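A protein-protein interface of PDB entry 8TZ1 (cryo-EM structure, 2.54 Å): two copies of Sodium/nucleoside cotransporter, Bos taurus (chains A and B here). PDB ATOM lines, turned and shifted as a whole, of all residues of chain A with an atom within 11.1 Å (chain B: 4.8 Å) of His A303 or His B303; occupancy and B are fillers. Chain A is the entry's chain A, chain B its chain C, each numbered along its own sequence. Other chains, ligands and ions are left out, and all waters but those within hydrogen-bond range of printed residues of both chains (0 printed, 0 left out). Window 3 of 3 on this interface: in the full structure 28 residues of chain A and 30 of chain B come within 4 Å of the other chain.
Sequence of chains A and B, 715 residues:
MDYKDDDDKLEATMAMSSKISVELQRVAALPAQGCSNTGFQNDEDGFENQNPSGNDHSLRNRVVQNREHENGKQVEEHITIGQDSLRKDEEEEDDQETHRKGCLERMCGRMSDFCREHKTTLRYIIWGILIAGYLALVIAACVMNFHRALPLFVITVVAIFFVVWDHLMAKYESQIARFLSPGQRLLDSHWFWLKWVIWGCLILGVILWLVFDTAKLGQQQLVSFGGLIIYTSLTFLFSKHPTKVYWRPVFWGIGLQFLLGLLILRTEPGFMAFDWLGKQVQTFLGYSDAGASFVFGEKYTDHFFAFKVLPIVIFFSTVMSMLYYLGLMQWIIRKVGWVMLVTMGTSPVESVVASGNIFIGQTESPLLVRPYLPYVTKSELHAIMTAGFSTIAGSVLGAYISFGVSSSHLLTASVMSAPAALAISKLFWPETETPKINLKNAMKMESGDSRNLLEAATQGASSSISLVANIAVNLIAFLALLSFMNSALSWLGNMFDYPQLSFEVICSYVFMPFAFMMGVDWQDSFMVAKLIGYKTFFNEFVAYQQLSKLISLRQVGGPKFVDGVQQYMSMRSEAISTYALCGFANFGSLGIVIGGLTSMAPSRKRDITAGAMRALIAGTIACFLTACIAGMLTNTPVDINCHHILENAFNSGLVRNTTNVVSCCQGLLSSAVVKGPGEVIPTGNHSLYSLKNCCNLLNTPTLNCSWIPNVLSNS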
ATOM      1  N   ASP A 289       9.669  -9.748  12.967  1.00  0.00           N
ATOM      2  CA  ASP A 289       9.427  -9.793  11.530  1.00  0.00           C
ATOM      3  C   ASP A 289      10.569  -9.157  10.751  1.00  0.00           C
ATOM      4  O   ASP A 289      10.815  -9.529   9.598  1.00  0.00           O
ATOM      5  CB  ASP A 289       8.109  -9.095  11.203  1.00  0.00           C
ATOM      6  CG  ASP A 289       6.911  -9.808  11.794  1.00  0.00           C
ATOM      7  OD1 ASP A 289       7.108 -10.846  12.460  1.00  0.00           O
ATOM      8  OD2 ASP A 289       5.774  -9.332  11.596  1.00  0.00           O
ATOM      9  N   ALA A 292      13.116 -11.941  10.379  1.00  0.00           N
ATOM     10  CA  ALA A 292      12.556 -13.009   9.560  1.00  0.00           C
ATOM     11  C   ALA A 292      12.480 -12.596   8.098  1.00  0.00           C
ATOM     12  O   ALA A 292      12.714 -13.412   7.200  1.00  0.00           O
ATOM     13  CB  ALA A 292      11.173 -13.393  10.078  1.00  0.00           C
ATOM     14  N   SER A 293      12.144 -11.332   7.838  1.00  0.00           N
ATOM     15  CA  SER A 293      12.027 -10.867   6.463  1.00  0.00           C
ATOM     16  C   SER A 293      13.364 -10.933   5.738  1.00  0.00           C
ATOM     17  O   SER A 293      13.420 -11.305   4.561  1.00  0.00           O
ATOM     18  CB  SER A 293      11.477  -9.444   6.440  1.00  0.00           C
ATOM     19  OG  SER A 293      11.289  -8.993   5.113  1.00  0.00           O
ATOM     20  N   VAL A 295      16.232 -12.834   6.583  1.00  0.00           N
ATOM     21  CA  VAL A 295      16.775 -14.184   6.476  1.00  0.00           C
ATOM     22  C   VAL A 295      15.957 -15.016   5.498  1.00  0.00           C
ATOM     23  O   VAL A 295      16.510 -15.726   4.650  1.00  0.00           O
ATOM     24  CB  VAL A 295      16.836 -14.843   7.865  1.00  0.00           C
ATOM     25  CG1 VAL A 295      17.351 -16.264   7.761  1.00  0.00           C
ATOM     26  CG2 VAL A 295      17.717 -14.038   8.792  1.00  0.00           C
ATOM     27  N   PHE A 296      14.630 -14.945   5.597  1.00  0.00           N
ATOM     28  CA  PHE A 296      13.743 -15.777   4.798  1.00  0.00           C
ATOM     29  C   PHE A 296      13.053 -15.005   3.682  1.00  0.00           C
ATOM     30  O   PHE A 296      12.201 -15.568   2.987  1.00  0.00           O
ATOM     31  CB  PHE A 296      12.703 -16.440   5.700  1.00  0.00           C
ATOM     32  CG  PHE A 296      13.299 -17.267   6.798  1.00  0.00           C
ATOM     33  CD1 PHE A 296      14.070 -18.378   6.505  1.00  0.00           C
ATOM     34  CD2 PHE A 296      13.089 -16.938   8.124  1.00  0.00           C
ATOM     35  CE1 PHE A 296      14.619 -19.138   7.512  1.00  0.00           C
ATOM     36  CE2 PHE A 296      13.636 -17.698   9.131  1.00  0.00           C
ATOM     37  CZ  PHE A 296      14.401 -18.797   8.824  1.00  0.00           C
ATOM     38  N   GLY A 297      13.400 -13.737   3.489  1.00  0.00           N
ATOM     39  CA  GLY A 297      12.851 -12.963   2.398  1.00  0.00           C
ATOM     40  C   GLY A 297      11.479 -12.402   2.707  1.00  0.00           C
ATOM     41  O   GLY A 297      10.892 -12.623   3.766  1.00  0.00           O
ATOM     42  N   GLU A 298      10.957 -11.649   1.738  1.00  0.00           N
ATOM     43  CA  GLU A 298       9.618 -11.087   1.844  1.00  0.00           C
ATOM     44  C   GLU A 298       8.527 -12.131   1.660  1.00  0.00           C
ATOM     45  O   GLU A 298       7.356 -11.832   1.919  1.00  0.00           O
ATOM     46  CB  GLU A 298       9.435  -9.972   0.814  1.00  0.00           C
ATOM     47  CG  GLU A 298      10.375  -8.796   1.009  1.00  0.00           C
ATOM     48  CD  GLU A 298      10.183  -7.718  -0.039  1.00  0.00           C
ATOM     49  OE1 GLU A 298       9.337  -7.906  -0.938  1.00  0.00           O
ATOM     50  OE2 GLU A 298      10.878  -6.682   0.035  1.00  0.00           O
ATOM     51  N   LYS A 299       8.878 -13.338   1.220  1.00  0.00           N
ATOM     52  CA  LYS A 299       7.940 -14.444   1.099  1.00  0.00           C
ATOM     53  C   LYS A 299       7.953 -15.344   2.328  1.00  0.00           C
ATOM     54  O   LYS A 299       7.489 -16.487   2.258  1.00  0.00           O
ATOM     55  CB  LYS A 299       8.248 -15.260  -0.155  1.00  0.00           C
ATOM     56  CG  LYS A 299       7.910 -14.554  -1.453  1.00  0.00           C
ATOM     57  CD  LYS A 299       8.269 -15.412  -2.650  1.00  0.00           C
ATOM     58  CE  LYS A 299       7.777 -14.800  -3.948  1.00  0.00           C
ATOM     59  NZ  LYS A 299       6.292 -14.770  -4.019  1.00  0.00           N
ATOM     60  N   TYR A 300       8.477 -14.852   3.452  1.00  0.00           N
ATOM     61  CA  TYR A 300       8.533 -15.662   4.663  1.00  0.00           C
ATOM     62  C   TYR A 300       7.147 -16.017   5.177  1.00  0.00           C
ATOM     63  O   TYR A 300       7.018 -16.932   5.998  1.00  0.00           O
ATOM     64  CB  TYR A 300       9.328 -14.931   5.748  1.00  0.00           C
ATOM     65  CG  TYR A 300       8.621 -13.740   6.353  1.00  0.00           C
ATOM     66  CD1 TYR A 300       8.413 -12.582   5.618  1.00  0.00           C
ATOM     67  CD2 TYR A 300       8.181 -13.766   7.668  1.00  0.00           C
ATOM     68  CE1 TYR A 300       7.772 -11.492   6.171  1.00  0.00           C
ATOM     69  CE2 TYR A 300       7.542 -12.681   8.228  1.00  0.00           C
ATOM     70  CZ  TYR A 300       7.341 -11.548   7.475  1.00  0.00           C
ATOM     71  OH  TYR A 300       6.705 -10.466   8.033  1.00  0.00           O
ATOM     72  N   THR A 301       6.109 -15.321   4.715  1.00  0.00           N
ATOM     73  CA  THR A 301       4.743 -15.637   5.102  1.00  0.00           C
ATOM     74  C   THR A 301       4.164 -16.810   4.325  1.00  0.00           C
ATOM     75  O   THR A 301       3.094 -17.306   4.691  1.00  0.00           O
ATOM     76  CB  THR A 301       3.848 -14.413   4.914  1.00  0.00           C
ATOM     77  OG1 THR A 301       4.078 -13.844   3.620  1.00  0.00           O
ATOM     78  CG2 THR A 301       4.141 -13.378   5.981  1.00  0.00           C
ATOM     79  N   ASP A 302       4.836 -17.260   3.263  1.00  0.00           N
ATOM     80  CA  ASP A 302       4.402 -18.474   2.582  1.00  0.00           C
ATOM     81  C   ASP A 302       4.499 -19.682   3.503  1.00  0.00           C
ATOM     82  O   ASP A 302       3.750 -20.652   3.339  1.00  0.00           O
ATOM     83  CB  ASP A 302       5.240 -18.697   1.323  1.00  0.00           C
ATOM     84  CG  ASP A 302       4.969 -17.661   0.253  1.00  0.00           C
ATOM     85  OD1 ASP A 302       4.140 -16.758   0.494  1.00  0.00           O
ATOM     86  OD2 ASP A 302       5.583 -17.748  -0.831  1.00  0.00           O
ATOM     87  N   HIS A 303       5.409 -19.637   4.475  1.00  0.00           N
ATOM     88  CA  HIS A 303       5.581 -20.684   5.481  1.00  0.00           C
ATOM     89  C   HIS A 303       5.441 -19.995   6.835  1.00  0.00           C
ATOM     90  O   HIS A 303       6.427 -19.551   7.427  1.00  0.00           O
ATOM     91  CB  HIS A 303       6.923 -21.378   5.322  1.00  0.00           C
ATOM     92  CG  HIS A 303       7.307 -21.623   3.897  1.00  0.00           C
ATOM     93  ND1 HIS A 303       6.715 -22.597   3.122  1.00  0.00           N
ATOM     94  CD2 HIS A 303       8.217 -21.013   3.102  1.00  0.00           C
ATOM     95  CE1 HIS A 303       7.246 -22.579   1.914  1.00  0.00           C
ATOM     96  NE2 HIS A 303       8.161 -21.627   1.875  1.00  0.00           N
ATOM     97  N   PHE A 304       4.202 -19.912   7.318  1.00  0.00           N
ATOM     98  CA  PHE A 304       3.905 -19.099   8.491  1.00  0.00           C
ATOM     99  C   PHE A 304       4.655 -19.596   9.722  1.00  0.00           C
ATOM    100  O   PHE A 304       5.493 -18.885  10.286  1.00  0.00           O
ATOM    101  CB  PHE A 304       2.394 -19.096   8.734  1.00  0.00           C
ATOM    102  CG  PHE A 304       1.976 -18.340   9.959  1.00  0.00           C
ATOM    103  CD1 PHE A 304       1.908 -16.958   9.946  1.00  0.00           C
ATOM    104  CD2 PHE A 304       1.637 -19.011  11.122  1.00  0.00           C
ATOM    105  CE1 PHE A 304       1.520 -16.261  11.070  1.00  0.00           C
ATOM    106  CE2 PHE A 304       1.248 -18.317  12.248  1.00  0.00           C
ATOM    107  CZ  PHE A 304       1.189 -16.942  12.221  1.00  0.00           C
ATOM    108  N   PHE A 305       4.368 -20.824  10.154  1.00  0.00           N
ATOM    109  CA  PHE A 305       4.876 -21.302  11.436  1.00  0.00           C
ATOM    110  C   PHE A 305       6.400 -21.284  11.477  1.00  0.00           C
ATOM    111  O   PHE A 305       7.006 -20.741  12.407  1.00  0.00           O
ATOM    112  CB  PHE A 305       4.349 -22.709  11.714  1.00  0.00           C
ATOM    113  CG  PHE A 305       4.784 -23.263  13.038  1.00  0.00           C
ATOM    114  CD1 PHE A 305       4.149 -22.877  14.206  1.00  0.00           C
ATOM    115  CD2 PHE A 305       5.830 -24.164  13.120  1.00  0.00           C
ATOM    116  CE1 PHE A 305       4.549 -23.381  15.423  1.00  0.00           C
ATOM    117  CE2 PHE A 305       6.230 -24.669  14.338  1.00  0.00           C
ATOM    118  CZ  PHE A 305       5.589 -24.277  15.488  1.00  0.00           C
ATOM    119  N   ALA A 306       7.040 -21.896  10.481  1.00  0.00           N
ATOM    120  CA  ALA A 306       8.489 -22.060  10.530  1.00  0.00           C
ATOM    121  C   ALA A 306       9.215 -20.725  10.422  1.00  0.00           C
ATOM    122  O   ALA A 306      10.158 -20.466  11.179  1.00  0.00           O
ATOM    123  CB  ALA A 306       8.942 -23.004   9.421  1.00  0.00           C
ATOM    124  N   PHE A 307       8.799 -19.869   9.494  1.00  0.00           N
ATOM    125  CA  PHE A 307       9.545 -18.662   9.166  1.00  0.00           C
ATOM    126  C   PHE A 307       9.026 -17.410   9.858  1.00  0.00           C
ATOM    127  O   PHE A 307       9.642 -16.350   9.715  1.00  0.00           O
ATOM    128  CB  PHE A 307       9.537 -18.435   7.652  1.00  0.00           C
ATOM    129  CG  PHE A 307      10.330 -19.451   6.873  1.00  0.00           C
ATOM    130  CD1 PHE A 307      11.036 -20.458   7.510  1.00  0.00           C
ATOM    131  CD2 PHE A 307      10.377 -19.385   5.493  1.00  0.00           C
ATOM    132  CE1 PHE A 307      11.761 -21.378   6.782  1.00  0.00           C
ATOM    133  CE2 PHE A 307      11.100 -20.302   4.768  1.00  0.00           C
ATOM    134  CZ  PHE A 307      11.791 -21.296   5.412  1.00  0.00           C
ATOM    135  N   LYS A 308       7.914 -17.488  10.588  1.00  0.00           N
ATOM    136  CA  LYS A 308       7.420 -16.316  11.302  1.00  0.00           C
ATOM    137  C   LYS A 308       7.265 -16.559  12.798  1.00  0.00           C
ATOM    138  O   LYS A 308       7.597 -15.686  13.606  1.00  0.00           O
ATOM    139  CB  LYS A 308       6.085 -15.860  10.716  1.00  0.00           C
ATOM    140  CG  LYS A 308       5.439 -14.742  11.501  1.00  0.00           C
ATOM    141  CD  LYS A 308       4.574 -13.874  10.619  1.00  0.00           C
ATOM    142  CE  LYS A 308       3.942 -12.743  11.409  1.00  0.00           C
ATOM    143  NZ  LYS A 308       3.419 -11.671  10.522  1.00  0.00           N
ATOM    144  N   VAL A 309       6.765 -17.732  13.182  1.00  0.00           N
ATOM    145  CA  VAL A 309       6.486 -17.992  14.591  1.00  0.00           C
ATOM    146  C   VAL A 309       7.763 -18.344  15.345  1.00  0.00           C
ATOM    147  O   VAL A 309       8.038 -17.789  16.414  1.00  0.00           O
ATOM    148  CB  VAL A 309       5.427 -19.099  14.725  1.00  0.00           C
ATOM    149  CG1 VAL A 309       5.316 -19.555  16.163  1.00  0.00           C
ATOM    150  CG2 VAL A 309       4.091 -18.594  14.234  1.00  0.00           C
ATOM    151  N   LEU A 310       8.555 -19.273  14.814  1.00  0.00           N
ATOM    152  CA  LEU A 310       9.777 -19.667  15.505  1.00  0.00           C
ATOM    153  C   LEU A 310      10.720 -18.495  15.745  1.00  0.00           C
ATOM    154  O   LEU A 310      11.308 -18.427  16.839  1.00  0.00           O
ATOM    155  CB  LEU A 310      10.471 -20.790  14.725  1.00  0.00           C
ATOM    156  CG  LEU A 310       9.650 -22.077  14.606  1.00  0.00           C
ATOM    157  CD1 LEU A 310      10.386 -23.110  13.785  1.00  0.00           C
ATOM    158  CD2 LEU A 310       9.310 -22.649  15.971  1.00  0.00           C
ATOM    159  N   PRO A 311      10.920 -17.568  14.807  1.00  0.00           N
ATOM    160  CA  PRO A 311      11.713 -16.371  15.120  1.00  0.00           C
ATOM    161  C   PRO A 311      11.223 -15.620  16.342  1.00  0.00           C
ATOM    162  O   PRO A 311      12.033 -15.000  17.042  1.00  0.00           O
ATOM    163  CB  PRO A 311      11.576 -15.532  13.847  1.00  0.00           C
ATOM    164  CG  PRO A 311      11.404 -16.530  12.771  1.00  0.00           C
ATOM    165  CD  PRO A 311      10.637 -17.676  13.366  1.00  0.00           C
ATOM    166  N   ILE A 312       9.919 -15.646  16.621  1.00  0.00           N
ATOM    167  CA  ILE A 312       9.415 -15.033  17.845  1.00  0.00           C
ATOM    168  C   ILE A 312      10.012 -15.725  19.061  1.00  0.00           C
ATOM    169  O   ILE A 312      10.393 -15.075  20.042  1.00  0.00           O
ATOM    170  CB  ILE A 312       7.876 -15.070  17.872  1.00  0.00           C
ATOM    171  CG1 ILE A 312       7.304 -14.295  16.687  1.00  0.00           C
ATOM    172  CG2 ILE A 312       7.363 -14.483  19.170  1.00  0.00           C
ATOM    173  CD1 ILE A 312       5.818 -14.469  16.500  1.00  0.00           C
ATOM    174  N   PHE A 403      -1.033 -17.696  17.583  1.00  0.00           N
ATOM    175  CA  PHE A 403      -2.130 -18.567  17.175  1.00  0.00           C
ATOM    176  C   PHE A 403      -3.469 -17.857  17.310  1.00  0.00           C
ATOM    177  O   PHE A 403      -4.343 -17.993  16.446  1.00  0.00           O
ATOM    178  CB  PHE A 403      -2.123 -19.847  18.011  1.00  0.00           C
ATOM    179  CG  PHE A 403      -0.941 -20.746  17.761  1.00  0.00           C
ATOM    180  CD1 PHE A 403      -0.176 -20.626  16.613  1.00  0.00           C
ATOM    181  CD2 PHE A 403      -0.603 -21.723  18.680  1.00  0.00           C
ATOM    182  CE1 PHE A 403       0.902 -21.458  16.396  1.00  0.00           C
ATOM    183  CE2 PHE A 403       0.475 -22.554  18.464  1.00  0.00           C
ATOM    184  CZ  PHE A 403       1.225 -22.422  17.323  1.00  0.00           C
ATOM    185  N   PHE B 296       5.531 -26.225   7.618  1.00  0.00           N
ATOM    186  CA  PHE B 296       6.012 -25.521   6.438  1.00  0.00           C
ATOM    187  C   PHE B 296       4.885 -24.962   5.581  1.00  0.00           C
ATOM    188  O   PHE B 296       5.149 -24.422   4.502  1.00  0.00           O
ATOM    189  CB  PHE B 296       6.896 -26.449   5.607  1.00  0.00           C
ATOM    190  CG  PHE B 296       8.066 -27.002   6.362  1.00  0.00           C
ATOM    191  CD1 PHE B 296       9.044 -26.162   6.862  1.00  0.00           C
ATOM    192  CD2 PHE B 296       8.189 -28.363   6.572  1.00  0.00           C
ATOM    193  CE1 PHE B 296      10.118 -26.670   7.557  1.00  0.00           C
ATOM    194  CE2 PHE B 296       9.264 -28.871   7.265  1.00  0.00           C
ATOM    195  CZ  PHE B 296      10.226 -28.023   7.758  1.00  0.00           C
ATOM    196  N   LYS B 299       2.330 -24.527   1.160  1.00  0.00           N
ATOM    197  CA  LYS B 299       3.293 -24.366   0.082  1.00  0.00           C
ATOM    198  C   LYS B 299       4.550 -25.193   0.309  1.00  0.00           C
ATOM    199  O   LYS B 299       5.586 -24.921  -0.309  1.00  0.00           O
ATOM    200  CB  LYS B 299       3.655 -22.890  -0.082  1.00  0.00           C
ATOM    201  CG  LYS B 299       2.544 -22.040  -0.664  1.00  0.00           C
ATOM    202  CD  LYS B 299       2.966 -20.588  -0.770  1.00  0.00           C
ATOM    203  CE  LYS B 299       1.938 -19.755  -1.511  1.00  0.00           C
ATOM    204  NZ  LYS B 299       1.826 -20.153  -2.939  1.00  0.00           N
ATOM    205  N   TYR B 300       4.484 -26.198   1.184  1.00  0.00           N
ATOM    206  CA  TYR B 300       5.653 -27.023   1.460  1.00  0.00           C
ATOM    207  C   TYR B 300       6.104 -27.801   0.233  1.00  0.00           C
ATOM    208  O   TYR B 300       7.235 -28.300   0.212  1.00  0.00           O
ATOM    209  CB  TYR B 300       5.358 -27.983   2.615  1.00  0.00           C
ATOM    210  CG  TYR B 300       4.410 -29.110   2.273  1.00  0.00           C
ATOM    211  CD1 TYR B 300       3.066 -28.867   2.032  1.00  0.00           C
ATOM    212  CD2 TYR B 300       4.856 -30.422   2.213  1.00  0.00           C
ATOM    213  CE1 TYR B 300       2.199 -29.894   1.724  1.00  0.00           C
ATOM    214  CE2 TYR B 300       3.996 -31.455   1.908  1.00  0.00           C
ATOM    215  CZ  TYR B 300       2.669 -31.185   1.666  1.00  0.00           C
ATOM    216  OH  TYR B 300       1.811 -32.214   1.362  1.00  0.00           O
ATOM    217  N   THR B 301       5.253 -27.914  -0.785  1.00  0.00           N
ATOM    218  CA  THR B 301       5.627 -28.584  -2.022  1.00  0.00           C
ATOM    219  C   THR B 301       6.448 -27.700  -2.948  1.00  0.00           C
ATOM    220  O   THR B 301       6.996 -28.204  -3.933  1.00  0.00           O
ATOM    221  CB  THR B 301       4.375 -29.062  -2.757  1.00  0.00           C
ATOM    222  OG1 THR B 301       3.416 -28.000  -2.816  1.00  0.00           O
ATOM    223  CG2 THR B 301       3.769 -30.252  -2.042  1.00  0.00           C
ATOM    224  N   ASP B 302       6.545 -26.400  -2.663  1.00  0.00           N
ATOM    225  CA  ASP B 302       7.444 -25.546  -3.430  1.00  0.00           C
ATOM    226  C   ASP B 302       8.892 -25.976  -3.251  1.00  0.00           C
ATOM    227  O   ASP B 302       9.721 -25.760  -4.141  1.00  0.00           O
ATOM    228  CB  ASP B 302       7.266 -24.087  -3.009  1.00  0.00           C
ATOM    229  CG  ASP B 302       5.922 -23.522  -3.420  1.00  0.00           C
ATOM    230  OD1 ASP B 302       5.120 -24.270  -4.018  1.00  0.00           O
ATOM    231  OD2 ASP B 302       5.668 -22.331  -3.146  1.00  0.00           O
ATOM    232  N   HIS B 303       9.211 -26.588  -2.111  1.00  0.00           N
ATOM    233  CA  HIS B 303      10.539 -27.122  -1.814  1.00  0.00           C
ATOM    234  C   HIS B 303      10.336 -28.597  -1.480  1.00  0.00           C
ATOM    235  O   HIS B 303      10.155 -28.966  -0.317  1.00  0.00           O
ATOM    236  CB  HIS B 303      11.194 -26.357  -0.676  1.00  0.00           C
ATOM    237  CG  HIS B 303      10.963 -24.879  -0.737  1.00  0.00           C
ATOM    238  ND1 HIS B 303      11.598 -24.062  -1.648  1.00  0.00           N
ATOM    239  CD2 HIS B 303      10.159 -24.072  -0.006  1.00  0.00           C
ATOM    240  CE1 HIS B 303      11.199 -22.817  -1.473  1.00  0.00           C
ATOM    241  NE2 HIS B 303      10.325 -22.794  -0.481  1.00  0.00           N
ATOM    242  N   PHE B 304      10.370 -29.435  -2.514  1.00  0.00           N
ATOM    243  CA  PHE B 304       9.984 -30.833  -2.363  1.00  0.00           C
ATOM    244  C   PHE B 304      10.894 -31.562  -1.378  1.00  0.00           C
ATOM    245  O   PHE B 304      10.444 -32.032  -0.328  1.00  0.00           O
ATOM    246  CB  PHE B 304      10.003 -31.515  -3.732  1.00  0.00           C
ATOM    247  CG  PHE B 304       9.684 -32.978  -3.690  1.00  0.00           C
ATOM    248  CD1 PHE B 304       8.375 -33.411  -3.568  1.00  0.00           C
ATOM    249  CD2 PHE B 304      10.690 -33.924  -3.785  1.00  0.00           C
ATOM    250  CE1 PHE B 304       8.078 -34.757  -3.531  1.00  0.00           C
ATOM    251  CE2 PHE B 304      10.397 -35.271  -3.750  1.00  0.00           C
ATOM    252  CZ  PHE B 304       9.091 -35.687  -3.623  1.00  0.00           C
ATOM    253  N   PHE B 305      12.182 -31.663  -1.701  1.00  0.00           N
ATOM    254  CA  PHE B 305      13.081 -32.517  -0.930  1.00  0.00           C
ATOM    255  C   PHE B 305      13.137 -32.094   0.533  1.00  0.00           C
ATOM    256  O   PHE B 305      12.960 -32.914   1.440  1.00  0.00           O
ATOM    257  CB  PHE B 305      14.478 -32.497  -1.550  1.00  0.00           C
ATOM    258  CG  PHE B 305      15.459 -33.387  -0.847  1.00  0.00           C
ATOM    259  CD1 PHE B 305      15.460 -34.752  -1.076  1.00  0.00           C
ATOM    260  CD2 PHE B 305      16.375 -32.866   0.047  1.00  0.00           C
ATOM    261  CE1 PHE B 305      16.357 -35.574  -0.430  1.00  0.00           C
ATOM    262  CE2 PHE B 305      17.274 -33.688   0.694  1.00  0.00           C
ATOM    263  CZ  PHE B 305      17.263 -35.040   0.455  1.00  0.00           C
ATOM    264  N   ALA B 306      13.406 -30.813   0.784  1.00  0.00           N
ATOM    265  CA  ALA B 306      13.635 -30.365   2.153  1.00  0.00           C
ATOM    266  C   ALA B 306      12.371 -30.455   2.998  1.00  0.00           C
ATOM    267  O   ALA B 306      12.415 -30.930   4.139  1.00  0.00           O
ATOM    268  CB  ALA B 306      14.172 -28.937   2.149  1.00  0.00           C
ATOM    269  N   PHE B 307      11.237 -30.008   2.464  1.00  0.00           N
ATOM    270  CA  PHE B 307      10.021 -29.855   3.249  1.00  0.00           C
ATOM    271  C   PHE B 307       9.052 -31.022   3.118  1.00  0.00           C
ATOM    272  O   PHE B 307       8.030 -31.029   3.810  1.00  0.00           O
ATOM    273  CB  PHE B 307       9.302 -28.562   2.857  1.00  0.00           C
ATOM    274  CG  PHE B 307      10.030 -27.306   3.257  1.00  0.00           C
ATOM    275  CD1 PHE B 307      11.220 -27.356   3.966  1.00  0.00           C
ATOM    276  CD2 PHE B 307       9.509 -26.068   2.930  1.00  0.00           C
ATOM    277  CE1 PHE B 307      11.871 -26.197   4.329  1.00  0.00           C
ATOM    278  CE2 PHE B 307      10.159 -24.912   3.294  1.00  0.00           C
ATOM    279  CZ  PHE B 307      11.338 -24.977   3.992  1.00  0.00           C
ATOM    280  N   LYS B 308       9.326 -31.994   2.251  1.00  0.00           N
ATOM    281  CA  LYS B 308       8.440 -33.148   2.139  1.00  0.00           C
ATOM    282  C   LYS B 308       9.162 -34.470   2.369  1.00  0.00           C
ATOM    283  O   LYS B 308       8.623 -35.365   3.028  1.00  0.00           O
ATOM    284  CB  LYS B 308       7.762 -33.167   0.770  1.00  0.00           C
ATOM    285  CG  LYS B 308       6.947 -34.415   0.525  1.00  0.00           C
ATOM    286  CD  LYS B 308       5.799 -34.150  -0.422  1.00  0.00           C
ATOM    287  CE  LYS B 308       4.973 -35.403  -0.651  1.00  0.00           C
ATOM    288  NZ  LYS B 308       3.646 -35.091  -1.245  1.00  0.00           N
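A ring nitrogen (NE2) of His B303 lies within hydrogen-bond range of a ring nitrogen (NE2) of His A303 (3.4 Å).
A ring nitrogen (ND1) of His A303 lies within hydrogen-bond range of the backbone carbonyl oxygen (O) of Phe B296, 2.8 Å away.
Among the printed residues, pairs that only touch across the chains: Asp A302 with Lys B299, His A303 with Lys B299, Phe A307 with Phe B307 and His A303 with Phe B307.
Ser A293 touches none of the printed residues of chain B.
Printed residues of chain B within 4 Å of Asp A302: Lys B299.
Of chain B, only Phe B296, Lys B299, His B303 and Phe B307 come within 4 Å of His A303.
Printed residues of chain B within 4 Å of Phe A307: Phe B307.
Printed residues of chain A within 4 Å of Phe B296: His A303.
Of the printed residues of chain A, Lys B299 touches Asp A302 (3.6 Å) and His A303 (3.6 Å).
Asp B302 touches none of the printed residues of chain A.
Of chain A, only His A303 comes within 4 Å of His B303.
Phe B307 touches just these residues of chain A: His A303 and Phe A307.
Printed residues of chain A that touch a printed residue of chain B: Asp A302, His A303 and Phe A307.
Of the 11 printed residues of chain B, 4 touch a printed residue of chain A.
Hydrophobic or aromatic side chains of chain B within 4 Å of the printed part of chain A: His B303 and Phe B307.
Along chain B the printed residues that touch a printed residue of chain A span positions 296 to 307.
Asp A302 touches Lys B299, but with the chains exchanged Lys A299 does not touch Asp B302 (7.4 Å).
His A303 touches Lys B299, but with the chains exchanged Lys A299 does not touch His B303 (7.4 Å).
His A303 touches Phe B307, but with the chains exchanged Phe A307 does not touch His B303 (5.9 Å).
Phe B307 touches its own counterpart, Phe A307.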
